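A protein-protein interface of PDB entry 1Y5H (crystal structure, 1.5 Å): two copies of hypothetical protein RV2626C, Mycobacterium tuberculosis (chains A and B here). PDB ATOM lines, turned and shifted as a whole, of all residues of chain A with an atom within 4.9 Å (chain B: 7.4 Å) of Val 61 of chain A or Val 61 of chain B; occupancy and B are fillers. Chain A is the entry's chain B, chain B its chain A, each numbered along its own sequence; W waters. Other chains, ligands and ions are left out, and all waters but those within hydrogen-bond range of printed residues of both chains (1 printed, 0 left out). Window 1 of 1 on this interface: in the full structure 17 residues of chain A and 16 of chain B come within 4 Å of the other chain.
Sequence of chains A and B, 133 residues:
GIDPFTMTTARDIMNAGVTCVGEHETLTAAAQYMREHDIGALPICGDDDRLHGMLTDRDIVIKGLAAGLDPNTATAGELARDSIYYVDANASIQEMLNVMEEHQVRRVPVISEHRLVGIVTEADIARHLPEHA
Ala 31 of chain A touches Val 61 of chain B, and with the chains exchanged Val 61 of chain A touches Ala 31 of chain B. Ala 31 of chain A touches Leu 65 of chain B, and with the chains exchanged Leu 65 of chain A touches Ala 31 of chain B. Ala 31 of chain A touches Ala 66 of chain B, and with the chains exchanged Ala 66 of chain A touches Ala 31 of chain B. Ile 60 of chain A touches Leu 65 of chain B, and with the chains exchanged Leu 65 of chain A touches Ile 60 of chain B. Positions printed for both chains: 31, 34, 57, 58, 59, 60, 61, 62, 63, 64, 65 and 66. Of the 21 pairs that touch across the chains among the printed residues, 17 have their exchanged pair printed and touching as well.
Of the printed residues of chain B, Ala 31 of chain A touches Val 61 (3.5 Å), Leu 65 (3.8 Å) and Ala 66 (3.5 Å). Of the printed residues of chain B, Arg 58 of chain A touches Met 34, Ile 39 and Asp 57. Val 61 of chain A touches three residues of chain B. Gly 64 of chain A touches none of the printed residues of chain B. Printed residues of chain A within 4 Å of Ala 31 of chain B: Val 61, Leu 65 and Ala 66. Printed residues of chain A within 4 Å of Ile 39 of chain B: Arg 58. Val 61 of chain B touches three residues of chain A. Ala 67 of chain B touches none of the printed residues of chain A. The nearest printed residue of chain A that does not touch Arg 35 of chain B is Arg 58 of chain A (4.9 Å).
O of Val 61 of chain A sits at hydrogen-bond distance from N of Ala 66 of chain A (2.8 Å). The backbone carbonyl oxygen of Val 61 of chain B is in hydrogen-bond range of the backbone NH of Ala 66 of chain B (2.8 Å). O of Met 34 of chain B is in hydrogen-bond range of N of Ile 39 of chain B (3.0 Å). The backbone NH of Leu 65 of chain A is in hydrogen-bond range of the backbone carbonyl oxygen of Ile 60 of chain A, 2.9 Å away. The backbone carbonyl oxygen (O) of Ile 60 of chain B lies within hydrogen-bond range of the backbone NH (N) of Leu 65 of chain B (2.9 Å).
The backbone carbonyl oxygen (O) of Met 34 of chain B is in hydrogen-bond range of the guanidinium group (NH2) of Arg 58 of chain A. The backbone carbonyl oxygen (O) of Ile 39 of chain B sits at hydrogen-bond distance from the guanidinium group (NH1) of Arg 58 of chain A, 2.9 Å away. The guanidinium group of Arg 35 of chain B sits at hydrogen-bond distance from the backbone carbonyl oxygen of Ala 66 of chain A (2.8 Å). The side-chain carboxylate (OD1) of Asp 57 of chain B is in salt-bridge range of the guanidinium group (NH1) of Arg 58 of chain A, at 2.9 Å. The side-chain carboxylate (OD2) of Asp 57 of chain A lies within salt-bridge range of the guanidinium group (NH1) of Arg 58 of chain B (3.0 Å).
Among the printed residues, pairs that only touch across the chains: Ala 31 of chain A with Val 61 of chain B (3.5 Å), Ala 31 of chain A with Leu 65 of chain B (3.8 Å), Ala 31 of chain A with Ala 66 of chain B (3.5 Å), Met 34 of chain A with Arg 58 of chain B (3.5 Å), Met 34 of chain A with Ile 62 of chain B (3.96 Å), Asp 57 of chain A with Val 61 of chain B (3.5 Å), Ile 60 of chain A with Leu 65 of chain B (3.5 Å), Val 61 of chain A with Ala 31 of chain B (3.6 Å), Val 61 of chain A with Asp 57 of chain B (3.4 Å), Val 61 of chain A with Val 61 of chain B (3.6 Å), Ile 62 of chain A with Met 34 of chain B (3.999 Å), Ile 62 of chain A with Arg 35 of chain B (3.7 Å), Leu 65 of chain A with Thr 28 of chain B (3.9 Å), Leu 65 of chain A with Ala 31 of chain B (3.8 Å), Leu 65 of chain A with Ile 60 of chain B (3.5 Å) and Ala 66 of chain A with Ala 31 of chain B (3.5 Å).
Water W1 lies within hydrogen-bond range of the backbone carbonyl oxygen (O) of Ile 62 of chain A and the guanidinium group (NH1) of Arg 35 of chain B.
Of the 22 printed residues of chain B, 12 touch a printed residue of chain A. Hydrophobic or aromatic side chains of chain B within 4 Å of the printed part of chain A: Ala 31, Ile 60, Val 61, Ile 62, Leu 65 and Ala 66. Along chain B the printed residues that touch a printed residue of chain A span positions 28 to 66. Of the 12 printed residues of chain A, 9 touch a printed residue of chain B. Among the printed residues, 21 pairs touch across the chains.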
ATOM      1  N   ALA A  31       1.575  28.053  -2.086  1.00  0.00           N
ATOM      2  CA  ALA A  31       0.508  29.006  -2.375  1.00  0.00           C
ATOM      3  C   ALA A  31       1.025  30.131  -3.278  1.00  0.00           C
ATOM      4  O   ALA A  31       0.324  30.572  -4.190  1.00  0.00           O
ATOM      5  CB  ALA A  31      -0.042  29.586  -1.076  1.00  0.00           C
ATOM      6  N   MET A  34       1.170  28.952  -6.813  1.00  0.00           N
ATOM      7  CA  MET A  34      -0.164  28.851  -7.393  1.00  0.00           C
ATOM      8  C   MET A  34      -0.670  30.222  -7.826  1.00  0.00           C
ATOM      9  O   MET A  34      -1.385  30.343  -8.822  1.00  0.00           O
ATOM     10  CB  MET A  34      -1.136  28.235  -6.391  1.00  0.00           C
ATOM     11  CG  MET A  34      -0.916  26.757  -6.164  1.00  0.00           C
ATOM     12  SD  MET A  34      -2.125  26.124  -4.822  1.00  0.00           S
ATOM     13  CE  MET A  34      -1.366  24.369  -4.526  1.00  0.00           C
ATOM     14  N   ASP A  57      -4.967  23.600  -4.222  1.00  0.00           N
ATOM     15  CA  ASP A  57      -5.232  24.721  -3.344  1.00  0.00           C
ATOM     16  C   ASP A  57      -6.162  24.267  -2.224  1.00  0.00           C
ATOM     17  O   ASP A  57      -5.961  24.622  -1.059  1.00  0.00           O
ATOM     18  CB  ASP A  57      -5.833  25.915  -4.113  1.00  0.00           C
ATOM     19  CG  ASP A  57      -6.933  25.521  -5.098  1.00  0.00           C
ATOM     20  OD1 ASP A  57      -7.446  24.380  -5.055  1.00  0.00           O
ATOM     21  OD2 ASP A  57      -7.288  26.391  -5.925  1.00  0.00           O
ATOM     22  N   ARG A  58      -7.166  23.465  -2.562  1.00  0.00           N
ATOM     23  CA  ARG A  58      -8.074  22.998  -1.531  1.00  0.00           C
ATOM     24  C   ARG A  58      -7.344  22.125  -0.507  1.00  0.00           C
ATOM     25  O   ARG A  58      -7.664  22.168   0.676  1.00  0.00           O
ATOM     26  CB  ARG A  58      -9.265  22.246  -2.136  1.00  0.00           C
ATOM     27  CG  ARG A  58     -10.335  21.934  -1.093  1.00  0.00           C
ATOM     28  CD  ARG A  58     -11.664  21.541  -1.713  1.00  0.00           C
ATOM     29  NE  ARG A  58     -12.626  21.160  -0.680  1.00  0.00           N
ATOM     30  CZ  ARG A  58     -13.278  22.013   0.107  1.00  0.00           C
ATOM     31  NH1 ARG A  58     -13.090  23.320  -0.011  1.00  0.00           N
ATOM     32  NH2 ARG A  58     -14.114  21.552   1.027  1.00  0.00           N
ATOM     33  N   ASP A  59      -6.350  21.349  -0.946  1.00  0.00           N
ATOM     34  CA  ASP A  59      -5.586  20.510  -0.017  1.00  0.00           C
ATOM     35  C   ASP A  59      -4.943  21.367   1.068  1.00  0.00           C
ATOM     36  O   ASP A  59      -4.914  20.991   2.240  1.00  0.00           O
ATOM     37  CB  ASP A  59      -4.435  19.775  -0.715  1.00  0.00           C
ATOM     38  CG  ASP A  59      -4.891  18.625  -1.571  1.00  0.00           C
ATOM     39  OD1 ASP A  59      -5.960  18.042  -1.289  1.00  0.00           O
ATOM     40  OD2 ASP A  59      -4.152  18.290  -2.524  1.00  0.00           O
ATOM     41  N   ILE A  60      -4.390  22.507   0.660  1.00  0.00           N
ATOM     42  CA  ILE A  60      -3.735  23.399   1.604  1.00  0.00           C
ATOM     43  C   ILE A  60      -4.719  23.867   2.670  1.00  0.00           C
ATOM     44  O   ILE A  60      -4.391  23.905   3.852  1.00  0.00           O
ATOM     45  CB  ILE A  60      -3.127  24.634   0.880  1.00  0.00           C
ATOM     46  CG1 ILE A  60      -1.990  24.179  -0.040  1.00  0.00           C
ATOM     47  CG2 ILE A  60      -2.586  25.638   1.901  1.00  0.00           C
ATOM     48  CD1 ILE A  60      -1.348  25.302  -0.821  1.00  0.00           C
ATOM     49  N   VAL A  61      -5.927  24.208   2.236  1.00  0.00           N
ATOM     50  CA  VAL A  61      -6.962  24.683   3.154  1.00  0.00           C
ATOM     51  C   VAL A  61      -7.527  23.573   4.032  1.00  0.00           C
ATOM     52  O   VAL A  61      -7.600  23.716   5.252  1.00  0.00           O
ATOM     53  CB  VAL A  61      -8.143  25.322   2.375  1.00  0.00           C
ATOM     54  CG1 VAL A  61      -9.260  25.734   3.341  1.00  0.00           C
ATOM     55  CG2 VAL A  61      -7.652  26.527   1.580  1.00  0.00           C
ATOM     56  N   ILE A  62      -7.917  22.467   3.406  1.00  0.00           N
ATOM     57  CA  ILE A  62      -8.535  21.352   4.119  1.00  0.00           C
ATOM     58  C   ILE A  62      -7.598  20.397   4.859  1.00  0.00           C
ATOM     59  O   ILE A  62      -7.844  20.058   6.022  1.00  0.00           O
ATOM     60  CB  ILE A  62      -9.426  20.546   3.155  1.00  0.00           C
ATOM     61  CG1 ILE A  62     -10.451  21.483   2.499  1.00  0.00           C
ATOM     62  CG2 ILE A  62     -10.126  19.422   3.900  1.00  0.00           C
ATOM     63  CD1 ILE A  62     -11.350  22.233   3.488  1.00  0.00           C
ATOM     64  N   LYS A  63      -6.529  19.958   4.199  1.00  0.00           N
ATOM     65  CA  LYS A  63      -5.582  19.045   4.836  1.00  0.00           C
ATOM     66  C   LYS A  63      -4.501  19.794   5.605  1.00  0.00           C
ATOM     67  O   LYS A  63      -3.766  19.206   6.401  1.00  0.00           O
ATOM     68  CB  LYS A  63      -4.921  18.147   3.789  1.00  0.00           C
ATOM     69  CG  LYS A  63      -5.884  17.238   3.054  1.00  0.00           C
ATOM     70  CD  LYS A  63      -5.153  16.393   2.021  1.00  0.00           C
ATOM     71  CE  LYS A  63      -6.105  15.439   1.315  1.00  0.00           C
ATOM     72  NZ  LYS A  63      -5.385  14.568   0.341  1.00  0.00           N
ATOM     73  N   GLY A  64      -4.409  21.095   5.362  1.00  0.00           N
ATOM     74  CA  GLY A  64      -3.412  21.899   6.038  1.00  0.00           C
ATOM     75  C   GLY A  64      -3.998  22.760   7.142  1.00  0.00           C
ATOM     76  O   GLY A  64      -3.978  22.372   8.310  1.00  0.00           O
ATOM     77  N   LEU A  65      -4.529  23.923   6.772  1.00  0.00           N
ATOM     78  CA  LEU A  65      -5.096  24.850   7.748  1.00  0.00           C
ATOM     79  C   LEU A  65      -6.186  24.244   8.623  1.00  0.00           C
ATOM     80  O   LEU A  65      -6.155  24.403   9.846  1.00  0.00           O
ATOM     81  CB  LEU A  65      -5.649  26.094   7.045  1.00  0.00           C
ATOM     82  CG  LEU A  65      -4.698  26.881   6.135  1.00  0.00           C
ATOM     83  CD1 LEU A  65      -5.413  28.125   5.601  1.00  0.00           C
ATOM     84  CD2 LEU A  65      -3.448  27.283   6.909  1.00  0.00           C
ATOM     85  N   ALA A  66      -7.140  23.554   8.007  1.00  0.00           N
ATOM     86  CA  ALA A  66      -8.246  22.960   8.761  1.00  0.00           C
ATOM     87  C   ALA A  66      -7.817  21.804   9.658  1.00  0.00           C
ATOM     88  O   ALA A  66      -8.556  21.414  10.569  1.00  0.00           O
ATOM     89  CB  ALA A  66      -9.343  22.503   7.809  1.00  0.00           C
ATOM     90  N   LEU B  27      -8.892  33.260   9.151  1.00  0.00           N
ATOM     91  CA  LEU B  27      -8.930  32.423   7.959  1.00  0.00           C
ATOM     92  C   LEU B  27      -8.807  30.956   8.357  1.00  0.00           C
ATOM     93  O   LEU B  27      -9.374  30.080   7.706  1.00  0.00           O
ATOM     94  CB  LEU B  27      -7.810  32.803   6.983  1.00  0.00           C
ATOM     95  CG  LEU B  27      -7.868  34.230   6.426  1.00  0.00           C
ATOM     96  CD1 LEU B  27      -6.735  34.418   5.410  1.00  0.00           C
ATOM     97  CD2 LEU B  27      -9.223  34.483   5.758  1.00  0.00           C
ATOM     98  N   THR B  28      -8.062  30.691   9.426  1.00  0.00           N
ATOM     99  CA  THR B  28      -7.913  29.322   9.899  1.00  0.00           C
ATOM    100  C   THR B  28      -9.283  28.810  10.339  1.00  0.00           C
ATOM    101  O   THR B  28      -9.653  27.672  10.057  1.00  0.00           O
ATOM    102  CB  THR B  28      -6.929  29.251  11.078  1.00  0.00           C
ATOM    103  OG1 THR B  28      -5.625  29.641  10.626  1.00  0.00           O
ATOM    104  CG2 THR B  28      -6.860  27.835  11.638  1.00  0.00           C
ATOM    105  N   ALA B  30     -12.179  29.847   9.256  1.00  0.00           N
ATOM    106  CA  ALA B  30     -12.986  29.687   8.051  1.00  0.00           C
ATOM    107  C   ALA B  30     -12.650  28.374   7.342  1.00  0.00           C
ATOM    108  O   ALA B  30     -13.531  27.712   6.798  1.00  0.00           O
ATOM    109  CB  ALA B  30     -12.763  30.866   7.109  1.00  0.00           C
ATOM    110  N   ALA B  31     -11.372  28.003   7.356  1.00  0.00           N
ATOM    111  CA  ALA B  31     -10.932  26.766   6.718  1.00  0.00           C
ATOM    112  C   ALA B  31     -11.591  25.581   7.409  1.00  0.00           C
ATOM    113  O   ALA B  31     -11.979  24.610   6.762  1.00  0.00           O
ATOM    114  CB  ALA B  31      -9.412  26.647   6.799  1.00  0.00           C
ATOM    115  N   GLN B  32     -11.713  25.666   8.729  1.00  0.00           N
ATOM    116  CA  GLN B  32     -12.350  24.597   9.494  1.00  0.00           C
ATOM    117  C   GLN B  32     -13.818  24.432   9.107  1.00  0.00           C
ATOM    118  O   GLN B  32     -14.322  23.312   9.034  1.00  0.00           O
ATOM    119  CB  GLN B  32     -12.227  24.881  10.991  1.00  0.00           C
ATOM    120  CG  GLN B  32     -10.788  24.845  11.475  1.00  0.00           C
ATOM    121  CD  GLN B  32     -10.611  25.375  12.883  1.00  0.00           C
ATOM    122  OE1 GLN B  32      -9.505  25.364  13.424  1.00  0.00           O
ATOM    123  NE2 GLN B  32     -11.696  25.847  13.484  1.00  0.00           N
ATOM    124  N   MET B  34     -15.136  25.108   6.198  1.00  0.00           N
ATOM    125  CA  MET B  34     -15.206  24.553   4.858  1.00  0.00           C
ATOM    126  C   MET B  34     -15.010  23.043   4.880  1.00  0.00           C
ATOM    127  O   MET B  34     -15.604  22.325   4.072  1.00  0.00           O
ATOM    128  CB  MET B  34     -14.157  25.207   3.967  1.00  0.00           C
ATOM    129  CG  MET B  34     -14.439  26.666   3.700  1.00  0.00           C
ATOM    130  SD  MET B  34     -13.004  27.410   2.682  1.00  0.00           S
ATOM    131  CE  MET B  34     -13.590  29.253   2.637  1.00  0.00           C
ATOM    132  N   ARG B  35     -14.176  22.565   5.802  1.00  0.00           N
ATOM    133  CA  ARG B  35     -13.942  21.130   5.918  1.00  0.00           C
ATOM    134  C   ARG B  35     -15.189  20.508   6.531  1.00  0.00           C
ATOM    135  O   ARG B  35     -15.648  19.458   6.089  1.00  0.00           O
ATOM    136  CB  ARG B  35     -12.734  20.833   6.814  1.00  0.00           C
ATOM    137  CG  ARG B  35     -12.469  19.332   6.974  1.00  0.00           C
ATOM    138  CD  ARG B  35     -11.220  19.024   7.791  1.00  0.00           C
ATOM    139  NE  ARG B  35     -11.327  19.462   9.179  1.00  0.00           N
ATOM    140  CZ  ARG B  35     -10.439  19.166  10.124  1.00  0.00           C
ATOM    141  NH1 ARG B  35      -9.377  18.426   9.829  1.00  0.00           N
ATOM    142  NH2 ARG B  35     -10.608  19.609  11.362  1.00  0.00           N
ATOM    143  N   ILE B  39     -17.431  22.366   1.639  1.00  0.00           N
ATOM    144  CA  ILE B  39     -17.772  23.369   0.639  1.00  0.00           C
ATOM    145  C   ILE B  39     -16.559  24.248   0.355  1.00  0.00           C
ATOM    146  O   ILE B  39     -15.599  24.266   1.131  1.00  0.00           O
ATOM    147  CB  ILE B  39     -18.941  24.269   1.103  1.00  0.00           C
ATOM    148  CG1 ILE B  39     -18.656  24.813   2.505  1.00  0.00           C
ATOM    149  CG2 ILE B  39     -20.245  23.488   1.059  1.00  0.00           C
ATOM    150  CD1 ILE B  39     -19.779  25.649   3.071  1.00  0.00           C
ATOM    151  N   THR B  56     -13.843  32.167  -0.532  1.00  0.00           N
ATOM    152  CA  THR B  56     -13.645  30.849  -1.118  1.00  0.00           C
ATOM    153  C   THR B  56     -12.352  30.225  -0.614  1.00  0.00           C
ATOM    154  O   THR B  56     -11.484  30.913  -0.065  1.00  0.00           O
ATOM    155  CB  THR B  56     -13.577  30.906  -2.658  1.00  0.00           C
ATOM    156  OG1 THR B  56     -12.407  31.632  -3.063  1.00  0.00           O
ATOM    157  CG2 THR B  56     -14.824  31.586  -3.219  1.00  0.00           C
ATOM    158  N   ASP B  57     -12.229  28.916  -0.796  1.00  0.00           N
ATOM    159  CA  ASP B  57     -11.024  28.235  -0.370  1.00  0.00           C
ATOM    160  C   ASP B  57      -9.816  28.776  -1.127  1.00  0.00           C
ATOM    161  O   ASP B  57      -8.754  28.983  -0.532  1.00  0.00           O
ATOM    162  CB  ASP B  57     -11.161  26.710  -0.550  1.00  0.00           C
ATOM    163  CG  ASP B  57     -11.720  26.301  -1.916  1.00  0.00           C
ATOM    164  OD1 ASP B  57     -12.011  25.097  -2.069  1.00  0.00           O
ATOM    165  OD2 ASP B  57     -11.866  27.146  -2.824  1.00  0.00           O
ATOM    166  N   ARG B  58      -9.979  29.036  -2.425  1.00  0.00           N
ATOM    167  CA  ARG B  58      -8.871  29.566  -3.208  1.00  0.00           C
ATOM    168  C   ARG B  58      -8.487  30.961  -2.718  1.00  0.00           C
ATOM    169  O   ARG B  58      -7.309  31.322  -2.741  1.00  0.00           O
ATOM    170  CB  ARG B  58      -9.205  29.608  -4.702  1.00  0.00           C
ATOM    171  CG  ARG B  58      -8.017  30.037  -5.540  1.00  0.00           C
ATOM    172  CD  ARG B  58      -8.197  29.756  -7.021  1.00  0.00           C
ATOM    173  NE  ARG B  58      -7.049  30.239  -7.787  1.00  0.00           N
ATOM    174  CZ  ARG B  58      -5.856  29.650  -7.826  1.00  0.00           C
ATOM    175  NH1 ARG B  58      -5.636  28.533  -7.145  1.00  0.00           N
ATOM    176  NH2 ARG B  58      -4.872  30.192  -8.535  1.00  0.00           N
ATOM    177  N   ASP B  59      -9.473  31.739  -2.267  1.00  0.00           N
ATOM    178  CA  ASP B  59      -9.210  33.084  -1.745  1.00  0.00           C
ATOM    179  C   ASP B  59      -8.215  33.006  -0.588  1.00  0.00           C
ATOM    180  O   ASP B  59      -7.287  33.802  -0.497  1.00  0.00           O
ATOM    181  CB  ASP B  59     -10.484  33.732  -1.182  1.00  0.00           C
ATOM    182  CG  ASP B  59     -11.387  34.305  -2.252  1.00  0.00           C
ATOM    183  OD1 ASP B  59     -10.951  34.440  -3.416  1.00  0.00           O
ATOM    184  OD2 ASP B  59     -12.546  34.641  -1.907  1.00  0.00           O
ATOM    185  N   ILE B  60      -8.446  32.057   0.312  1.00  0.00           N
ATOM    186  CA  ILE B  60      -7.584  31.880   1.474  1.00  0.00           C
ATOM    187  C   ILE B  60      -6.147  31.596   1.048  1.00  0.00           C
ATOM    188  O   ILE B  60      -5.200  32.110   1.637  1.00  0.00           O
ATOM    189  CB  ILE B  60      -8.099  30.730   2.362  1.00  0.00           C
ATOM    190  CG1 ILE B  60      -9.450  31.132   2.977  1.00  0.00           C
ATOM    191  CG2 ILE B  60      -7.074  30.397   3.455  1.00  0.00           C
ATOM    192  CD1 ILE B  60     -10.074  30.047   3.844  1.00  0.00           C
ATOM    193  N   VAL B  61      -5.995  30.793   0.004  1.00  0.00           N
ATOM    194  CA  VAL B  61      -4.669  30.444  -0.486  1.00  0.00           C
ATOM    195  C   VAL B  61      -4.011  31.573  -1.275  1.00  0.00           C
ATOM    196  O   VAL B  61      -2.861  31.929  -1.010  1.00  0.00           O
ATOM    197  CB  VAL B  61      -4.733  29.188  -1.394  1.00  0.00           C
ATOM    198  CG1 VAL B  61      -3.356  28.887  -1.993  1.00  0.00           C
ATOM    199  CG2 VAL B  61      -5.219  27.987  -0.590  1.00  0.00           C
ATOM    200  N   ILE B  62      -4.748  32.138  -2.230  1.00  0.00           N
ATOM    201  CA  ILE B  62      -4.214  33.184  -3.106  1.00  0.00           C
ATOM    202  C   ILE B  62      -4.157  34.596  -2.534  1.00  0.00           C
ATOM    203  O   ILE B  62      -3.149  35.287  -2.687  1.00  0.00           O
ATOM    204  CB  ILE B  62      -5.005  33.233  -4.436  1.00  0.00           C
ATOM    205  CG1 ILE B  62      -4.985  31.854  -5.103  1.00  0.00           C
ATOM    206  CG2 ILE B  62      -4.426  34.300  -5.356  1.00  0.00           C
ATOM    207  CD1 ILE B  62      -3.593  31.310  -5.389  1.00  0.00           C
ATOM    208  N   LYS B  63      -5.239  35.030  -1.897  1.00  0.00           N
ATOM    209  CA  LYS B  63      -5.288  36.366  -1.318  1.00  0.00           C
ATOM    210  C   LYS B  63      -4.801  36.365   0.123  1.00  0.00           C
ATOM    211  O   LYS B  63      -4.510  37.415   0.683  1.00  0.00           O
ATOM    212  CB  LYS B  63      -6.716  36.915  -1.374  1.00  0.00           C
ATOM    213  CG  LYS B  63      -7.262  37.124  -2.782  1.00  0.00           C
ATOM    214  CD  LYS B  63      -8.672  37.700  -2.739  1.00  0.00           C
ATOM    215  CE  LYS B  63      -9.240  37.885  -4.137  1.00  0.00           C
ATOM    216  NZ  LYS B  63     -10.605  38.476  -4.096  1.00  0.00           N
ATOM    217  N   GLY B  64      -4.717  35.181   0.717  1.00  0.00           N
ATOM    218  CA  GLY B  64      -4.262  35.077   2.088  1.00  0.00           C
ATOM    219  C   GLY B  64      -2.819  34.621   2.188  1.00  0.00           C
ATOM    220  O   GLY B  64      -1.908  35.440   2.298  1.00  0.00           O
ATOM    221  N   LEU B  65      -2.610  33.310   2.129  1.00  0.00           N
ATOM    222  CA  LEU B  65      -1.266  32.751   2.252  1.00  0.00           C
ATOM    223  C   LEU B  65      -0.253  33.295   1.254  1.00  0.00           C
ATOM    224  O   LEU B  65       0.869  33.640   1.635  1.00  0.00           O
ATOM    225  CB  LEU B  65      -1.309  31.227   2.138  1.00  0.00           C
ATOM    226  CG  LEU B  65      -2.181  30.464   3.144  1.00  0.00           C
ATOM    227  CD1 LEU B  65      -1.977  28.967   2.954  1.00  0.00           C
ATOM    228  CD2 LEU B  65      -1.817  30.870   4.568  1.00  0.00           C
ATOM    229  N   ALA B  66      -0.639  33.378  -0.014  1.00  0.00           N
ATOM    230  CA  ALA B  66       0.275  33.869  -1.050  1.00  0.00           C
ATOM    231  C   ALA B  66       0.528  35.367  -0.967  1.00  0.00           C
ATOM    232  O   ALA B  66       1.457  35.876  -1.603  1.00  0.00           O
ATOM    233  CB  ALA B  66      -0.259  33.509  -2.436  1.00  0.00           C
ATOM    234  N   ALA B  67      -0.284  36.075  -0.185  1.00  0.00           N
ATOM    235  CA  ALA B  67      -0.123  37.516  -0.039  1.00  0.00           C
ATOM    236  C   ALA B  67       0.579  37.867   1.270  1.00  0.00           C
ATOM    237  O   ALA B  67       0.548  39.015   1.710  1.00  0.00           O
ATOM    238  CB  ALA B  67      -1.482  38.211  -0.110  1.00  0.00           C
ATOM    239  N   GLY B  68       1.196  36.872   1.896  1.00  0.00           N
ATOM    240  CA  GLY B  68       1.924  37.110   3.130  1.00  0.00           C
ATOM    241  C   GLY B  68       1.107  37.318   4.392  1.00  0.00           C
ATOM    242  O   GLY B  68       1.633  37.801   5.397  1.00  0.00           O
ATOM    243  N   LEU B  79     -10.777  39.410   3.380  1.00  0.00           N
ATOM    244  CA  LEU B  79     -10.716  38.837   2.041  1.00  0.00           C
ATOM    245  C   LEU B  79     -12.079  38.806   1.349  1.00  0.00           C
ATOM    246  O   LEU B  79     -12.169  38.976   0.132  1.00  0.00           O
ATOM    247  CB  LEU B  79     -10.147  37.414   2.096  1.00  0.00           C
ATOM    248  CG  LEU B  79      -8.638  37.257   2.324  1.00  0.00           C
ATOM    249  CD1 LEU B  79      -8.233  37.864   3.652  1.00  0.00           C
ATOM    250  CD2 LEU B  79      -8.272  35.784   2.268  1.00  0.00           C
HETATM  251  O   HOH W   1      -8.277  17.631   7.216  1.00  0.00           O
